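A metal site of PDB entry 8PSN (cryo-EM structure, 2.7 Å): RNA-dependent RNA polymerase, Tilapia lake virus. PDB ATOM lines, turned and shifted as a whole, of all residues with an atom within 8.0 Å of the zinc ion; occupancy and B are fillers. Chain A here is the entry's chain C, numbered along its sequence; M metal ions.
O of Glu 232 sits close to NE2 of His 184 (3.4 Å).
The backbone NH (N) of His 184 is in hydrogen-bond range of the backbone carbonyl oxygen (O) of Ile 177 (2.9 Å).
Within 4 Å of the zinc ion: His 184, His 191, Cys 233 and Cys 235.
The nearest printed residue that does not touch the zinc ion is Pro 234 (4.9 Å).
The zinc ion is bound by a ring nitrogen (NE2) of His 191, a ring nitrogen (ND1) of His 184, the side-chain sulfur (SG) of Cys 233 and the side-chain sulfur (SG) of Cys 235.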
ATOM      1  N   PHE A 175      19.493 -28.161   3.646  1.00  0.00           N
ATOM      2  CA  PHE A 175      20.566 -29.009   4.137  1.00  0.00           C
ATOM      3  C   PHE A 175      20.891 -28.677   5.590  1.00  0.00           C
ATOM      4  O   PHE A 175      20.613 -27.584   6.081  1.00  0.00           O
ATOM      5  CB  PHE A 175      21.833 -28.893   3.261  1.00  0.00           C
ATOM      6  CG  PHE A 175      22.526 -27.561   3.352  1.00  0.00           C
ATOM      7  CD1 PHE A 175      23.335 -27.248   4.435  1.00  0.00           C
ATOM      8  CD2 PHE A 175      22.421 -26.641   2.330  1.00  0.00           C
ATOM      9  CE1 PHE A 175      23.982 -26.037   4.516  1.00  0.00           C
ATOM     10  CE2 PHE A 175      23.068 -25.425   2.389  1.00  0.00           C
ATOM     11  CZ  PHE A 175      23.854 -25.122   3.487  1.00  0.00           C
ATOM     12  N   ILE A 177      24.317 -29.216   8.134  1.00  0.00           N
ATOM     13  CA  ILE A 177      25.732 -29.547   8.180  1.00  0.00           C
ATOM     14  C   ILE A 177      26.275 -29.213   9.559  1.00  0.00           C
ATOM     15  O   ILE A 177      25.913 -28.195  10.149  1.00  0.00           O
ATOM     16  CB  ILE A 177      26.542 -28.807   7.099  1.00  0.00           C
ATOM     17  CG1 ILE A 177      26.019 -29.114   5.705  1.00  0.00           C
ATOM     18  CG2 ILE A 177      28.013 -29.185   7.180  1.00  0.00           C
ATOM     19  CD1 ILE A 177      26.578 -28.190   4.631  1.00  0.00           C
ATOM     20  N   ILE A 179      29.180 -27.762  11.462  1.00  0.00           N
ATOM     21  CA  ILE A 179      30.364 -26.923  11.326  1.00  0.00           C
ATOM     22  C   ILE A 179      30.942 -26.735  12.723  1.00  0.00           C
ATOM     23  O   ILE A 179      30.303 -26.122  13.589  1.00  0.00           O
ATOM     24  CB  ILE A 179      30.042 -25.565  10.673  1.00  0.00           C
ATOM     25  CG1 ILE A 179      29.391 -25.762   9.300  1.00  0.00           C
ATOM     26  CG2 ILE A 179      31.299 -24.716  10.564  1.00  0.00           C
ATOM     27  CD1 ILE A 179      30.350 -26.294   8.244  1.00  0.00           C
ATOM     28  N   PHE A 182      28.584 -26.418  15.926  1.00  0.00           N
ATOM     29  CA  PHE A 182      27.225 -25.948  15.696  1.00  0.00           C
ATOM     30  C   PHE A 182      26.611 -26.619  14.467  1.00  0.00           C
ATOM     31  O   PHE A 182      27.293 -26.817  13.461  1.00  0.00           O
ATOM     32  CB  PHE A 182      27.195 -24.424  15.523  1.00  0.00           C
ATOM     33  CG  PHE A 182      27.444 -23.668  16.791  1.00  0.00           C
ATOM     34  CD1 PHE A 182      28.734 -23.348  17.181  1.00  0.00           C
ATOM     35  CD2 PHE A 182      26.391 -23.270  17.598  1.00  0.00           C
ATOM     36  CE1 PHE A 182      28.969 -22.649  18.355  1.00  0.00           C
ATOM     37  CE2 PHE A 182      26.620 -22.579  18.769  1.00  0.00           C
ATOM     38  CZ  PHE A 182      27.907 -22.266  19.144  1.00  0.00           C
ATOM     39  N   TRP A 183      25.328 -26.954  14.554  1.00  0.00           N
ATOM     40  CA  TRP A 183      24.584 -27.509  13.427  1.00  0.00           C
ATOM     41  C   TRP A 183      23.949 -26.357  12.655  1.00  0.00           C
ATOM     42  O   TRP A 183      23.067 -25.663  13.182  1.00  0.00           O
ATOM     43  CB  TRP A 183      23.524 -28.489  13.913  1.00  0.00           C
ATOM     44  CG  TRP A 183      24.086 -29.783  14.396  1.00  0.00           C
ATOM     45  CD1 TRP A 183      24.382 -30.124  15.690  1.00  0.00           C
ATOM     46  CD2 TRP A 183      24.404 -30.937  13.599  1.00  0.00           C
ATOM     47  NE1 TRP A 183      24.877 -31.402  15.747  1.00  0.00           N
ATOM     48  CE2 TRP A 183      24.899 -31.921  14.473  1.00  0.00           C
ATOM     49  CE3 TRP A 183      24.326 -31.217  12.242  1.00  0.00           C
ATOM     50  CZ2 TRP A 183      25.297 -33.177  14.029  1.00  0.00           C
ATOM     51  CZ3 TRP A 183      24.727 -32.461  11.792  1.00  0.00           C
ATOM     52  CH2 TRP A 183      25.209 -33.424  12.686  1.00  0.00           C
ATOM     53  N   HIS A 184      24.389 -26.148  11.418  1.00  0.00           N
ATOM     54  CA  HIS A 184      23.847 -25.109  10.549  1.00  0.00           C
ATOM     55  C   HIS A 184      22.772 -25.721   9.669  1.00  0.00           C
ATOM     56  O   HIS A 184      23.026 -26.686   8.943  1.00  0.00           O
ATOM     57  CB  HIS A 184      24.953 -24.483   9.703  1.00  0.00           C
ATOM     58  CG  HIS A 184      25.922 -23.664  10.482  1.00  0.00           C
ATOM     59  ND1 HIS A 184      26.132 -22.322  10.234  1.00  0.00           N
ATOM     60  CD2 HIS A 184      26.747 -23.984  11.514  1.00  0.00           C
ATOM     61  CE1 HIS A 184      27.045 -21.855  11.072  1.00  0.00           C
ATOM     62  NE2 HIS A 184      27.422 -22.847  11.863  1.00  0.00           N
ATOM     63  N   MET A 185      21.566 -25.158   9.740  1.00  0.00           N
ATOM     64  CA  MET A 185      20.418 -25.589   8.943  1.00  0.00           C
ATOM     65  C   MET A 185      20.097 -24.459   7.967  1.00  0.00           C
ATOM     66  O   MET A 185      19.705 -23.367   8.391  1.00  0.00           O
ATOM     67  CB  MET A 185      19.226 -25.914   9.830  1.00  0.00           C
ATOM     68  CG  MET A 185      19.548 -26.812  11.006  1.00  0.00           C
ATOM     69  SD  MET A 185      19.877 -25.895  12.521  1.00  0.00           S
ATOM     70  CE  MET A 185      18.245 -25.863  13.262  1.00  0.00           C
ATOM     71  N   TYR A 186      20.259 -24.726   6.674  1.00  0.00           N
ATOM     72  CA  TYR A 186      20.030 -23.731   5.637  1.00  0.00           C
ATOM     73  C   TYR A 186      18.966 -24.248   4.676  1.00  0.00           C
ATOM     74  O   TYR A 186      19.139 -25.293   4.057  1.00  0.00           O
ATOM     75  CB  TYR A 186      21.317 -23.415   4.870  1.00  0.00           C
ATOM     76  CG  TYR A 186      21.233 -22.177   4.020  1.00  0.00           C
ATOM     77  CD1 TYR A 186      20.741 -20.980   4.539  1.00  0.00           C
ATOM     78  CD2 TYR A 186      21.640 -22.188   2.692  1.00  0.00           C
ATOM     79  CE1 TYR A 186      20.659 -19.846   3.758  1.00  0.00           C
ATOM     80  CE2 TYR A 186      21.565 -21.058   1.906  1.00  0.00           C
ATOM     81  CZ  TYR A 186      21.069 -19.891   2.445  1.00  0.00           C
ATOM     82  OH  TYR A 186      20.988 -18.757   1.664  1.00  0.00           O
ATOM     83  N   HIS A 191      18.267 -19.098   7.505  1.00  0.00           N
ATOM     84  CA  HIS A 191      19.435 -19.792   8.019  1.00  0.00           C
ATOM     85  C   HIS A 191      19.347 -19.837   9.546  1.00  0.00           C
ATOM     86  O   HIS A 191      19.014 -18.830  10.179  1.00  0.00           O
ATOM     87  CB  HIS A 191      20.722 -19.088   7.590  1.00  0.00           C
ATOM     88  CG  HIS A 191      21.960 -19.636   8.246  1.00  0.00           C
ATOM     89  ND1 HIS A 191      22.422 -19.167   9.455  1.00  0.00           N
ATOM     90  CD2 HIS A 191      22.821 -20.597   7.856  1.00  0.00           C
ATOM     91  CE1 HIS A 191      23.523 -19.817   9.786  1.00  0.00           C
ATOM     92  NE2 HIS A 191      23.785 -20.695   8.824  1.00  0.00           N
ATOM     93  N   PHE A 192      19.640 -20.995  10.125  1.00  0.00           N
ATOM     94  CA  PHE A 192      19.552 -21.166  11.558  1.00  0.00           C
ATOM     95  C   PHE A 192      20.741 -21.984  12.059  1.00  0.00           C
ATOM     96  O   PHE A 192      21.358 -22.735  11.313  1.00  0.00           O
ATOM     97  CB  PHE A 192      18.238 -21.839  11.967  1.00  0.00           C
ATOM     98  CG  PHE A 192      17.049 -20.926  11.917  1.00  0.00           C
ATOM     99  CD1 PHE A 192      16.870 -19.960  12.890  1.00  0.00           C
ATOM    100  CD2 PHE A 192      16.114 -21.035  10.904  1.00  0.00           C
ATOM    101  CE1 PHE A 192      15.778 -19.110  12.848  1.00  0.00           C
ATOM    102  CE2 PHE A 192      15.015 -20.192  10.861  1.00  0.00           C
ATOM    103  CZ  PHE A 192      14.852 -19.228  11.838  1.00  0.00           C
ATOM    104  N   VAL A 193      21.037 -21.813  13.344  1.00  0.00           N
ATOM    105  CA  VAL A 193      22.112 -22.535  14.016  1.00  0.00           C
ATOM    106  C   VAL A 193      21.561 -23.185  15.264  1.00  0.00           C
ATOM    107  O   VAL A 193      20.725 -22.597  15.967  1.00  0.00           O
ATOM    108  CB  VAL A 193      23.289 -21.591  14.365  1.00  0.00           C
ATOM    109  CG1 VAL A 193      24.271 -22.299  15.284  1.00  0.00           C
ATOM    110  CG2 VAL A 193      23.981 -21.119  13.096  1.00  0.00           C
ATOM    111  N   ALA A 230      26.686 -18.366  15.921  1.00  0.00           N
ATOM    112  CA  ALA A 230      27.863 -18.942  15.300  1.00  0.00           C
ATOM    113  C   ALA A 230      28.637 -17.852  14.561  1.00  0.00           C
ATOM    114  O   ALA A 230      28.075 -16.828  14.154  1.00  0.00           O
ATOM    115  CB  ALA A 230      27.493 -20.073  14.330  1.00  0.00           C
ATOM    116  N   ALA A 231      29.933 -18.104  14.366  1.00  0.00           N
ATOM    117  CA  ALA A 231      30.821 -17.173  13.680  1.00  0.00           C
ATOM    118  C   ALA A 231      31.137 -17.628  12.266  1.00  0.00           C
ATOM    119  O   ALA A 231      30.921 -16.889  11.310  1.00  0.00           O
ATOM    120  CB  ALA A 231      32.114 -16.989  14.497  1.00  0.00           C
ATOM    121  N   GLU A 232      31.665 -18.848  12.107  1.00  0.00           N
ATOM    122  CA  GLU A 232      31.925 -19.390  10.785  1.00  0.00           C
ATOM    123  C   GLU A 232      30.641 -19.982  10.217  1.00  0.00           C
ATOM    124  O   GLU A 232      29.959 -20.766  10.891  1.00  0.00           O
ATOM    125  CB  GLU A 232      33.021 -20.457  10.848  1.00  0.00           C
ATOM    126  CG  GLU A 232      34.422 -19.889  10.978  1.00  0.00           C
ATOM    127  CD  GLU A 232      35.482 -20.975  11.031  1.00  0.00           C
ATOM    128  OE1 GLU A 232      35.111 -22.163  11.104  1.00  0.00           O
ATOM    129  OE2 GLU A 232      36.681 -20.644  10.988  1.00  0.00           O
ATOM    130  N   CYS A 233      30.317 -19.616   8.975  1.00  0.00           N
ATOM    131  CA  CYS A 233      29.075 -20.058   8.373  1.00  0.00           C
ATOM    132  C   CYS A 233      29.162 -19.972   6.848  1.00  0.00           C
ATOM    133  O   CYS A 233      28.681 -18.999   6.263  1.00  0.00           O
ATOM    134  CB  CYS A 233      27.902 -19.218   8.873  1.00  0.00           C
ATOM    135  SG  CYS A 233      26.313 -19.585   8.095  1.00  0.00           S
ATOM    136  N   PRO A 234      29.769 -20.971   6.185  1.00  0.00           N
ATOM    137  CA  PRO A 234      29.789 -20.992   4.718  1.00  0.00           C
ATOM    138  C   PRO A 234      28.572 -21.676   4.112  1.00  0.00           C
ATOM    139  O   PRO A 234      28.683 -22.537   3.236  1.00  0.00           O
ATOM    140  CB  PRO A 234      31.090 -21.762   4.437  1.00  0.00           C
ATOM    141  CG  PRO A 234      31.095 -22.819   5.537  1.00  0.00           C
ATOM    142  CD  PRO A 234      30.287 -22.238   6.716  1.00  0.00           C
ATOM    143  N   CYS A 235      27.383 -21.293   4.575  1.00  0.00           N
ATOM    144  CA  CYS A 235      26.167 -21.929   4.089  1.00  0.00           C
ATOM    145  C   CYS A 235      25.823 -21.469   2.677  1.00  0.00           C
ATOM    146  O   CYS A 235      25.392 -22.280   1.850  1.00  0.00           O
ATOM    147  CB  CYS A 235      25.009 -21.627   5.040  1.00  0.00           C
ATOM    148  SG  CYS A 235      24.895 -22.781   6.426  1.00  0.00           S
ATOM    149  N   LYS A 236      26.014 -20.179   2.378  1.00  0.00           N
ATOM    150  CA  LYS A 236      25.741 -19.692   1.030  1.00  0.00           C
ATOM    151  C   LYS A 236      26.660 -20.350   0.009  1.00  0.00           C
ATOM    152  O   LYS A 236      26.215 -20.713  -1.090  1.00  0.00           O
ATOM    153  CB  LYS A 236      25.889 -18.172   0.984  1.00  0.00           C
ATOM    154  CG  LYS A 236      24.567 -17.410   0.966  1.00  0.00           C
ATOM    155  CD  LYS A 236      23.925 -17.351   2.344  1.00  0.00           C
ATOM    156  CE  LYS A 236      23.215 -16.025   2.569  1.00  0.00           C
ATOM    157  NZ  LYS A 236      22.838 -15.836   3.999  1.00  0.00           N
ATOM    158  N   VAL A 238      28.256 -23.348   0.082  1.00  0.00           N
ATOM    159  CA  VAL A 238      27.877 -24.736  -0.185  1.00  0.00           C
ATOM    160  C   VAL A 238      26.518 -24.797  -0.883  1.00  0.00           C
ATOM    161  O   VAL A 238      26.297 -25.671  -1.723  1.00  0.00           O
ATOM    162  CB  VAL A 238      27.883 -25.561   1.115  1.00  0.00           C
ATOM    163  CG1 VAL A 238      29.214 -25.411   1.832  1.00  0.00           C
ATOM    164  CG2 VAL A 238      26.738 -25.163   2.022  1.00  0.00           C
HETATM  165 ZN    ZN M   1      25.495 -21.709   8.385  1.00  0.00          ZN
